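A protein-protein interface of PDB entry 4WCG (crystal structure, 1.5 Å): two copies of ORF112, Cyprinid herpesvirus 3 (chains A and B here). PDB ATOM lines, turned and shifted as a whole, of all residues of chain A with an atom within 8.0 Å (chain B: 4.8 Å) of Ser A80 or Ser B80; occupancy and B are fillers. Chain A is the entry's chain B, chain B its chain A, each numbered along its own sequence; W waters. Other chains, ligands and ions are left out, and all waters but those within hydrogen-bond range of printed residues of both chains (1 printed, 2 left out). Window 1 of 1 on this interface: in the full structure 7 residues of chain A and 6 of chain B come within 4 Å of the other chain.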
ATOM      1  N   ASN A  43       7.823  25.192  12.720  1.00  0.00           N
ATOM      2  CA  ASN A  43       8.947  24.254  12.695  1.00  0.00           C
ATOM      3  C   ASN A  43       9.542  24.176  11.300  1.00  0.00           C
ATOM      4  O   ASN A  43      10.758  24.236  11.121  1.00  0.00           O
ATOM      5  CB  ASN A  43       8.515  22.863  13.142  1.00  0.00           C
ATOM      6  CG  ASN A  43       8.336  22.758  14.636  1.00  0.00           C
ATOM      7  OD1 ASN A  43       8.853  23.578  15.399  1.00  0.00           O
ATOM      8  ND2 ASN A  43       7.601  21.733  15.067  1.00  0.00           N
ATOM      9  N   ASN A  73      12.662  30.442  19.688  1.00  0.00           N
ATOM     10  CA  ASN A  73      13.316  29.606  20.689  1.00  0.00           C
ATOM     11  C   ASN A  73      12.410  28.516  21.232  1.00  0.00           C
ATOM     12  O   ASN A  73      12.875  27.390  21.471  1.00  0.00           O
ATOM     13  CB  ASN A  73      13.856  30.461  21.834  1.00  0.00           C
ATOM     14  CG  ASN A  73      15.265  30.934  21.550  1.00  0.00           C
ATOM     15  OD1 ASN A  73      15.992  30.247  20.846  1.00  0.00           O
ATOM     16  ND2 ASN A  73      15.649  32.090  22.075  1.00  0.00           N
ATOM     17  N   ARG A  74      11.131  28.803  21.458  1.00  0.00           N
ATOM     18  CA  ARG A  74      10.250  27.752  21.945  1.00  0.00           C
ATOM     19  C   ARG A  74      10.247  26.567  20.973  1.00  0.00           C
ATOM     20  O   ARG A  74      10.286  25.400  21.391  1.00  0.00           O
ATOM     21  CB  ARG A  74       8.842  28.298  22.172  1.00  0.00           C
ATOM     22  CG  ARG A  74       7.908  27.256  22.757  1.00  0.00           C
ATOM     23  CD  ARG A  74       6.599  27.839  23.253  1.00  0.00           C
ATOM     24  NE  ARG A  74       5.782  28.322  22.150  1.00  0.00           N
ATOM     25  CZ  ARG A  74       5.690  29.594  21.778  1.00  0.00           C
ATOM     26  NH1 ARG A  74       6.369  30.534  22.422  1.00  0.00           N
ATOM     27  NH2 ARG A  74       4.911  29.927  20.762  1.00  0.00           N
ATOM     28  N   HIS A  75      10.216  26.868  19.678  1.00  0.00           N
ATOM     29  CA  HIS A  75      10.182  25.822  18.666  1.00  0.00           C
ATOM     30  C   HIS A  75      11.538  25.126  18.501  1.00  0.00           C
ATOM     31  O   HIS A  75      11.583  23.902  18.343  1.00  0.00           O
ATOM     32  CB  HIS A  75       9.702  26.411  17.341  1.00  0.00           C
ATOM     33  CG  HIS A  75       8.230  26.702  17.338  1.00  0.00           C
ATOM     34  ND1 HIS A  75       7.671  27.759  18.035  1.00  0.00           N
ATOM     35  CD2 HIS A  75       7.191  26.031  16.786  1.00  0.00           C
ATOM     36  CE1 HIS A  75       6.359  27.742  17.875  1.00  0.00           C
ATOM     37  NE2 HIS A  75       6.040  26.706  17.119  1.00  0.00           N
ATOM     38  N   LEU A  76      12.626  25.888  18.535  1.00  0.00           N
ATOM     39  CA  LEU A  76      13.957  25.278  18.439  1.00  0.00           C
ATOM     40  C   LEU A  76      14.185  24.270  19.557  1.00  0.00           C
ATOM     41  O   LEU A  76      14.630  23.139  19.319  1.00  0.00           O
ATOM     42  CB  LEU A  76      15.052  26.344  18.501  1.00  0.00           C
ATOM     43  CG  LEU A  76      15.251  27.165  17.239  1.00  0.00           C
ATOM     44  CD1 LEU A  76      16.119  28.372  17.563  1.00  0.00           C
ATOM     45  CD2 LEU A  76      15.897  26.296  16.147  1.00  0.00           C
ATOM     46  N   TYR A  77      13.921  24.680  20.791  1.00  0.00           N
ATOM     47  CA  TYR A  77      14.195  23.782  21.904  1.00  0.00           C
ATOM     48  C   TYR A  77      13.324  22.530  21.848  1.00  0.00           C
ATOM     49  O   TYR A  77      13.802  21.433  22.140  1.00  0.00           O
ATOM     50  CB  TYR A  77      14.035  24.529  23.227  1.00  0.00           C
ATOM     51  CG  TYR A  77      15.261  25.371  23.569  1.00  0.00           C
ATOM     52  CD1 TYR A  77      15.378  26.695  23.138  1.00  0.00           C
ATOM     53  CD2 TYR A  77      16.297  24.840  24.350  1.00  0.00           C
ATOM     54  CE1 TYR A  77      16.499  27.451  23.449  1.00  0.00           C
ATOM     55  CE2 TYR A  77      17.407  25.591  24.657  1.00  0.00           C
ATOM     56  CZ  TYR A  77      17.511  26.891  24.203  1.00  0.00           C
ATOM     57  OH  TYR A  77      18.632  27.606  24.560  1.00  0.00           O
ATOM     58  N   ARG A  78      12.055  22.666  21.487  1.00  0.00           N
ATOM     59  CA  ARG A  78      11.233  21.465  21.389  1.00  0.00           C
ATOM     60  C   ARG A  78      11.732  20.558  20.255  1.00  0.00           C
ATOM     61  O   ARG A  78      11.804  19.342  20.428  1.00  0.00           O
ATOM     62  CB  ARG A  78       9.760  21.825  21.199  1.00  0.00           C
ATOM     63  CG  ARG A  78       9.096  22.384  22.464  1.00  0.00           C
ATOM     64  CD  ARG A  78       9.298  21.489  23.704  1.00  0.00           C
ATOM     65  NE  ARG A  78       8.615  22.041  24.875  1.00  0.00           N
ATOM     66  CZ  ARG A  78       8.687  21.578  26.125  1.00  0.00           C
ATOM     67  NH1 ARG A  78       9.431  20.518  26.440  1.00  0.00           N
ATOM     68  NH2 ARG A  78       7.997  22.191  27.078  1.00  0.00           N
ATOM     69  N   MET A  79      12.105  21.135  19.114  1.00  0.00           N
ATOM     70  CA  MET A  79      12.604  20.309  18.010  1.00  0.00           C
ATOM     71  C   MET A  79      13.897  19.613  18.402  1.00  0.00           C
ATOM     72  O   MET A  79      14.180  18.524  17.913  1.00  0.00           O
ATOM     73  CB  MET A  79      12.844  21.130  16.735  1.00  0.00           C
ATOM     74  CG  MET A  79      11.590  21.340  15.925  1.00  0.00           C
ATOM     75  SD  MET A  79      11.956  21.897  14.242  1.00  0.00           S
ATOM     76  CE  MET A  79      12.393  23.600  14.546  1.00  0.00           C
ATOM     77  N   SER A  80      14.680  20.225  19.283  1.00  0.00           N
ATOM     78  CA  SER A  80      15.960  19.621  19.674  1.00  0.00           C
ATOM     79  C   SER A  80      15.774  18.351  20.499  1.00  0.00           C
ATOM     80  O   SER A  80      16.653  17.494  20.518  1.00  0.00           O
ATOM     81  CB  SER A  80      16.834  20.609  20.463  1.00  0.00           C
ATOM     82  OG  SER A  80      16.368  20.788  21.782  1.00  0.00           O
ATOM     83  N   GLU A  81      14.635  18.229  21.174  1.00  0.00           N
ATOM     84  CA  GLU A  81      14.373  17.073  22.049  1.00  0.00           C
ATOM     85  C   GLU A  81      14.479  15.775  21.293  1.00  0.00           C
ATOM     86  O   GLU A  81      15.030  14.797  21.808  1.00  0.00           O
ATOM     87  CB  GLU A  81      12.990  17.160  22.676  1.00  0.00           C
ATOM     88  CG  GLU A  81      12.853  18.344  23.574  1.00  0.00           C
ATOM     89  CD  GLU A  81      11.463  18.543  24.125  1.00  0.00           C
ATOM     90  OE1 GLU A  81      10.551  17.722  23.866  1.00  0.00           O
ATOM     91  OE2 GLU A  81      11.296  19.551  24.833  1.00  0.00           O
ATOM     92  N   ASP A  82      13.922  15.746  20.090  1.00  0.00           N
ATOM     93  CA  ASP A  82      13.882  14.513  19.323  1.00  0.00           C
ATOM     94  C   ASP A  82      14.841  14.557  18.138  1.00  0.00           C
ATOM     95  O   ASP A  82      14.785  13.710  17.259  1.00  0.00           O
ATOM     96  CB  ASP A  82      12.449  14.215  18.860  1.00  0.00           C
ATOM     97  CG  ASP A  82      11.792  15.403  18.172  1.00  0.00           C
ATOM     98  OD1 ASP A  82      12.498  16.166  17.486  1.00  0.00           O
ATOM     99  OD2 ASP A  82      10.562  15.567  18.314  1.00  0.00           O
ATOM    100  N   GLY A  83      15.724  15.546  18.133  1.00  0.00           N
ATOM    101  CA  GLY A  83      16.830  15.603  17.201  1.00  0.00           C
ATOM    102  C   GLY A  83      16.638  16.279  15.855  1.00  0.00           C
ATOM    103  O   GLY A  83      17.447  16.079  14.956  1.00  0.00           O
ATOM    104  N   ARG A  84      15.591  17.079  15.703  1.00  0.00           N
ATOM    105  CA  ARG A  84      15.359  17.733  14.422  1.00  0.00           C
ATOM    106  C   ARG A  84      16.262  18.942  14.234  1.00  0.00           C
ATOM    107  O   ARG A  84      16.508  19.363  13.110  1.00  0.00           O
ATOM    108  CB  ARG A  84      13.891  18.136  14.284  1.00  0.00           C
ATOM    109  CG  ARG A  84      13.003  16.956  13.954  1.00  0.00           C
ATOM    110  CD  ARG A  84      11.540  17.338  14.013  1.00  0.00           C
ATOM    111  NE  ARG A  84      11.076  17.465  15.390  1.00  0.00           N
ATOM    112  CZ  ARG A  84       9.980  18.124  15.744  1.00  0.00           C
ATOM    113  NH1 ARG A  84       9.253  18.736  14.822  1.00  0.00           N
ATOM    114  NH2 ARG A  84       9.625  18.184  17.017  1.00  0.00           N
ATOM    115  N   VAL A  85      16.739  19.508  15.338  1.00  0.00           N
ATOM    116  CA  VAL A  85      17.778  20.541  15.285  1.00  0.00           C
ATOM    117  C   VAL A  85      18.733  20.253  16.432  1.00  0.00           C
ATOM    118  O   VAL A  85      18.415  19.445  17.306  1.00  0.00           O
ATOM    119  CB  VAL A  85      17.249  21.971  15.418  1.00  0.00           C
ATOM    120  CG1 VAL A  85      16.271  22.312  14.292  1.00  0.00           C
ATOM    121  CG2 VAL A  85      16.575  22.181  16.761  1.00  0.00           C
ATOM    122  N   ARG A  86      19.900  20.894  16.424  1.00  0.00           N
ATOM    123  CA  ARG A  86      20.900  20.673  17.458  1.00  0.00           C
ATOM    124  C   ARG A  86      21.503  22.011  17.819  1.00  0.00           C
ATOM    125  O   ARG A  86      21.692  22.863  16.944  1.00  0.00           O
ATOM    126  CB  ARG A  86      21.992  19.696  16.973  1.00  0.00           C
ATOM    127  CG  ARG A  86      22.947  19.206  18.058  1.00  0.00           C
ATOM    128  CD  ARG A  86      24.034  18.329  17.450  1.00  0.00           C
ATOM    129  NE  ARG A  86      23.478  17.278  16.600  1.00  0.00           N
ATOM    130  CZ  ARG A  86      24.183  16.588  15.708  1.00  0.00           C
ATOM    131  NH1 ARG A  86      25.474  16.846  15.539  1.00  0.00           N
ATOM    132  NH2 ARG A  86      23.597  15.647  14.977  1.00  0.00           N
ATOM    133  N   LYS A  87      21.780  22.198  19.101  1.00  0.00           N
ATOM    134  CA  LYS A  87      22.406  23.410  19.590  1.00  0.00           C
ATOM    135  C   LYS A  87      23.883  23.181  19.854  1.00  0.00           C
ATOM    136  O   LYS A  87      24.298  22.081  20.250  1.00  0.00           O
ATOM    137  CB  LYS A  87      21.724  23.869  20.879  1.00  0.00           C
ATOM    138  CG  LYS A  87      22.021  25.289  21.278  1.00  0.00           C
ATOM    139  CD  LYS A  87      21.367  25.617  22.633  1.00  0.00           C
ATOM    140  CE  LYS A  87      22.170  25.054  23.793  1.00  0.00           C
ATOM    141  NZ  LYS A  87      23.437  25.817  23.989  1.00  0.00           N
ATOM    142  N   TRP A  94      22.403  27.353  16.501  1.00  0.00           N
ATOM    143  CA  TRP A  94      21.620  26.188  16.099  1.00  0.00           C
ATOM    144  C   TRP A  94      21.981  25.659  14.728  1.00  0.00           C
ATOM    145  O   TRP A  94      22.306  26.440  13.829  1.00  0.00           O
ATOM    146  CB  TRP A  94      20.133  26.544  16.129  1.00  0.00           C
ATOM    147  CG  TRP A  94      19.694  26.922  17.485  1.00  0.00           C
ATOM    148  CD1 TRP A  94      19.727  28.169  18.050  1.00  0.00           C
ATOM    149  CD2 TRP A  94      19.138  26.047  18.456  1.00  0.00           C
ATOM    150  NE1 TRP A  94      19.242  28.107  19.334  1.00  0.00           N
ATOM    151  CE2 TRP A  94      18.870  26.820  19.604  1.00  0.00           C
ATOM    152  CE3 TRP A  94      18.854  24.680  18.476  1.00  0.00           C
ATOM    153  CZ2 TRP A  94      18.318  26.272  20.753  1.00  0.00           C
ATOM    154  CZ3 TRP A  94      18.300  24.134  19.633  1.00  0.00           C
ATOM    155  CH2 TRP A  94      18.037  24.935  20.745  1.00  0.00           C
ATOM    156  N   TYR A  95      21.913  24.329  14.589  1.00  0.00           N
ATOM    157  CA  TYR A  95      22.319  23.608  13.376  1.00  0.00           C
ATOM    158  C   TYR A  95      21.313  22.539  13.013  1.00  0.00           C
ATOM    159  O   TYR A  95      20.579  22.052  13.865  1.00  0.00           O
ATOM    160  CB  TYR A  95      23.664  22.894  13.568  1.00  0.00           C
ATOM    161  CG  TYR A  95      24.756  23.701  14.193  1.00  0.00           C
ATOM    162  CD1 TYR A  95      24.872  23.798  15.570  1.00  0.00           C
ATOM    163  CD2 TYR A  95      25.695  24.355  13.407  1.00  0.00           C
ATOM    164  CE1 TYR A  95      25.885  24.535  16.149  1.00  0.00           C
ATOM    165  CE2 TYR A  95      26.712  25.092  13.974  1.00  0.00           C
ATOM    166  CZ  TYR A  95      26.806  25.182  15.343  1.00  0.00           C
ATOM    167  OH  TYR A  95      27.823  25.920  15.907  1.00  0.00           O
ATOM    168  N   LEU B  76      18.280  15.180  31.248  1.00  0.00           N
ATOM    169  CA  LEU B  76      17.961  14.590  29.939  1.00  0.00           C
ATOM    170  C   LEU B  76      17.602  15.664  28.925  1.00  0.00           C
ATOM    171  O   LEU B  76      18.114  15.690  27.798  1.00  0.00           O
ATOM    172  CB  LEU B  76      16.794  13.594  30.041  1.00  0.00           C
ATOM    173  CG  LEU B  76      17.117  12.242  30.677  1.00  0.00           C
ATOM    174  CD1 LEU B  76      15.823  11.514  31.058  1.00  0.00           C
ATOM    175  CD2 LEU B  76      17.922  11.395  29.679  1.00  0.00           C
ATOM    176  N   TYR B  77      16.704  16.563  29.310  1.00  0.00           N
ATOM    177  CA  TYR B  77      16.279  17.576  28.359  1.00  0.00           C
ATOM    178  C   TYR B  77      17.421  18.525  27.990  1.00  0.00           C
ATOM    179  O   TYR B  77      17.541  18.916  26.836  1.00  0.00           O
ATOM    180  CB  TYR B  77      15.073  18.348  28.898  1.00  0.00           C
ATOM    181  CG  TYR B  77      13.759  17.611  28.681  1.00  0.00           C
ATOM    182  CD1 TYR B  77      13.300  16.671  29.602  1.00  0.00           C
ATOM    183  CD2 TYR B  77      13.011  17.831  27.539  1.00  0.00           C
ATOM    184  CE1 TYR B  77      12.106  16.002  29.396  1.00  0.00           C
ATOM    185  CE2 TYR B  77      11.826  17.169  27.316  1.00  0.00           C
ATOM    186  CZ  TYR B  77      11.375  16.249  28.250  1.00  0.00           C
ATOM    187  OH  TYR B  77      10.187  15.601  28.006  1.00  0.00           O
ATOM    188  N   ARG B  78      18.268  18.899  28.943  1.00  0.00           N
ATOM    189  CA  ARG B  78      19.384  19.750  28.559  1.00  0.00           C
ATOM    190  C   ARG B  78      20.374  19.009  27.649  1.00  0.00           C
ATOM    191  O   ARG B  78      20.898  19.607  26.702  1.00  0.00           O
ATOM    192  CB  ARG B  78      20.073  20.306  29.793  1.00  0.00           C
ATOM    193  CG  ARG B  78      19.200  21.337  30.530  1.00  0.00           C
ATOM    194  CD  ARG B  78      18.691  22.489  29.628  1.00  0.00           C
ATOM    195  NE  ARG B  78      18.025  23.531  30.413  1.00  0.00           N
ATOM    196  CZ  ARG B  78      17.492  24.653  29.923  1.00  0.00           C
ATOM    197  NH1 ARG B  78      17.520  24.919  28.614  1.00  0.00           N
ATOM    198  NH2 ARG B  78      16.925  25.526  30.752  1.00  0.00           N
ATOM    199  N   MET B  79      20.617  17.720  27.917  1.00  0.00           N
ATOM    200  CA  MET B  79      21.498  16.938  27.026  1.00  0.00           C
ATOM    201  C   MET B  79      20.898  16.768  25.635  1.00  0.00           C
ATOM    202  O   MET B  79      21.637  16.646  24.647  1.00  0.00           O
ATOM    203  CB  MET B  79      21.810  15.562  27.618  1.00  0.00           C
ATOM    204  CG  MET B  79      22.953  15.628  28.619  1.00  0.00           C
ATOM    205  SD  MET B  79      23.604  14.010  29.063  1.00  0.00           S
ATOM    206  CE  MET B  79      22.217  13.338  29.993  1.00  0.00           C
ATOM    207  N   SER B  80      19.574  16.765  25.539  1.00  0.00           N
ATOM    208  CA  SER B  80      18.948  16.574  24.243  1.00  0.00           C
ATOM    209  C   SER B  80      19.185  17.798  23.346  1.00  0.00           C
ATOM    210  O   SER B  80      19.167  17.688  22.125  1.00  0.00           O
ATOM    211  CB  SER B  80      17.447  16.299  24.391  1.00  0.00           C
ATOM    212  OG  SER B  80      16.711  17.478  24.682  1.00  0.00           O
ATOM    213  N   GLU B  81      19.416  18.972  23.936  1.00  0.00           N
ATOM    214  CA  GLU B  81      19.632  20.180  23.149  1.00  0.00           C
ATOM    215  C   GLU B  81      20.818  20.044  22.210  1.00  0.00           C
ATOM    216  O   GLU B  81      20.735  20.455  21.062  1.00  0.00           O
ATOM    217  CB  GLU B  81      19.838  21.405  24.049  1.00  0.00           C
ATOM    218  CG  GLU B  81      18.617  21.716  24.881  1.00  0.00           C
ATOM    219  CD  GLU B  81      18.864  22.735  25.964  1.00  0.00           C
ATOM    220  OE1 GLU B  81      19.961  23.333  26.017  1.00  0.00           O
ATOM    221  OE2 GLU B  81      17.929  22.936  26.763  1.00  0.00           O
ATOM    222  N   ASP B  82      21.920  19.473  22.705  1.00  0.00           N
ATOM    223  CA  ASP B  82      23.103  19.339  21.864  1.00  0.00           C
ATOM    224  C   ASP B  82      23.302  17.920  21.368  1.00  0.00           C
ATOM    225  O   ASP B  82      24.375  17.579  20.867  1.00  0.00           O
ATOM    226  CB  ASP B  82      24.365  19.828  22.590  1.00  0.00           C
ATOM    227  CG  ASP B  82      24.567  19.182  23.947  1.00  0.00           C
ATOM    228  OD1 ASP B  82      23.579  18.902  24.643  1.00  0.00           O
ATOM    229  OD2 ASP B  82      25.740  18.980  24.329  1.00  0.00           O
ATOM    230  N   GLY B  83      22.267  17.100  21.488  1.00  0.00           N
ATOM    231  CA  GLY B  83      22.261  15.791  20.851  1.00  0.00           C
ATOM    232  C   GLY B  83      22.980  14.669  21.574  1.00  0.00           C
ATOM    233  O   GLY B  83      23.288  13.636  20.971  1.00  0.00           O
ATOM    234  N   VAL B  85      21.622  12.994  24.103  1.00  0.00           N
ATOM    235  CA  VAL B  85      20.537  12.021  24.182  1.00  0.00           C
ATOM    236  C   VAL B  85      19.451  12.465  23.207  1.00  0.00           C
ATOM    237  O   VAL B  85      19.452  13.609  22.726  1.00  0.00           O
ATOM    238  CB  VAL B  85      19.931  11.897  25.618  1.00  0.00           C
ATOM    239  CG1 VAL B  85      20.987  11.482  26.616  1.00  0.00           C
ATOM    240  CG2 VAL B  85      19.286  13.205  26.061  1.00  0.00           C
ATOM    241  N   TRP B  94      13.826   7.542  26.136  1.00  0.00           N
ATOM    242  CA  TRP B  94      15.100   8.181  25.795  1.00  0.00           C
ATOM    243  C   TRP B  94      16.118   7.218  25.193  1.00  0.00           C
ATOM    244  O   TRP B  94      16.276   6.066  25.635  1.00  0.00           O
ATOM    245  CB  TRP B  94      15.705   8.848  27.040  1.00  0.00           C
ATOM    246  CG  TRP B  94      14.806   9.935  27.541  1.00  0.00           C
ATOM    247  CD1 TRP B  94      13.752   9.814  28.421  1.00  0.00           C
ATOM    248  CD2 TRP B  94      14.839  11.310  27.151  1.00  0.00           C
ATOM    249  NE1 TRP B  94      13.147  11.025  28.591  1.00  0.00           N
ATOM    250  CE2 TRP B  94      13.793  11.967  27.834  1.00  0.00           C
ATOM    251  CE3 TRP B  94      15.657  12.054  26.298  1.00  0.00           C
ATOM    252  CZ2 TRP B  94      13.555  13.339  27.689  1.00  0.00           C
ATOM    253  CZ3 TRP B  94      15.417  13.395  26.147  1.00  0.00           C
ATOM    254  CH2 TRP B  94      14.375  14.034  26.847  1.00  0.00           C
HETATM  255  O   HOH W   1       8.380  16.973  26.464  1.00  0.00           O
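The backbone carbonyl oxygen (O) of Glu B81 is in hydrogen-bond range of the backbone NH (N) of Lys A87 (2.8 Å). O of Ser B80 lies close to O of Ser A80 (3.0 Å).
Tyr A77 touches Glu B81, and with the chains exchanged Glu A81 touches Tyr B77. Ser A80 touches its own counterpart, Ser B80. Ser A80 touches Glu B81, and with the chains exchanged Glu A81 touches Ser B80. 10 positions are printed for both chains. Of the 9 pairs that touch across the chains among the printed residues, 5 have their exchanged pair printed and touching as well.
Of the 18 printed residues of chain A, 5 touch a printed residue of chain B. Hydrophobic or aromatic side chains of chain A within 4 Å of the printed part of chain B: Tyr A77.
Of the printed residues of chain B, Ser A80 touches Ser B80 and Glu B81. Of chain A, only Ser A80 (3.0 Å) and Glu A81 (3.5 Å) come within 4 Å of Ser B80. Printed residues of chain B within 4 Å of Lys A87: Glu B81 and Asp B82. Printed residues of chain B within 4 Å of Arg A86: Glu B81 and Asp B82. Arg B78 touches none of the printed residues of chain A.
Water W1 lies within hydrogen-bond range of OH of Tyr B77 (2.7 Å) and OE1 of Glu A81 (3.5 Å).
The backbone carbonyl oxygen (O) of Tyr B77 sits at hydrogen-bond distance from the side-chain hydroxyl (OG) of Ser B80 (2.7 Å). NH1 of Arg B78 is in salt-bridge range of OE2 of Glu B81, at 2.7 Å. The backbone carbonyl oxygen (O) of Tyr A77 sits at hydrogen-bond distance from the side-chain hydroxyl (OG) of Ser A80 (2.7 Å). The guanidinium group of Arg A78 lies within salt-bridge range of the side-chain carboxylate of Glu A81, 2.6 Å away. N of Tyr A95 sits at hydrogen-bond distance from O of Arg A86, at 2.8 Å.
CE2 of Tyr A77 touches OE2 of Glu B81, 3.4 Å away. Glu B81 touches Ser A80. Glu A81 touches Tyr B77 (OE2 to CE2, 3.5 Å). Glu A81 touches Ser B80. Arg A86 touches Glu B81. Arg A86 touches Asp B82 (CD to O, 3.5 Å). Lys A87 touches Asp B82 (O to CB, 3.2 Å).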
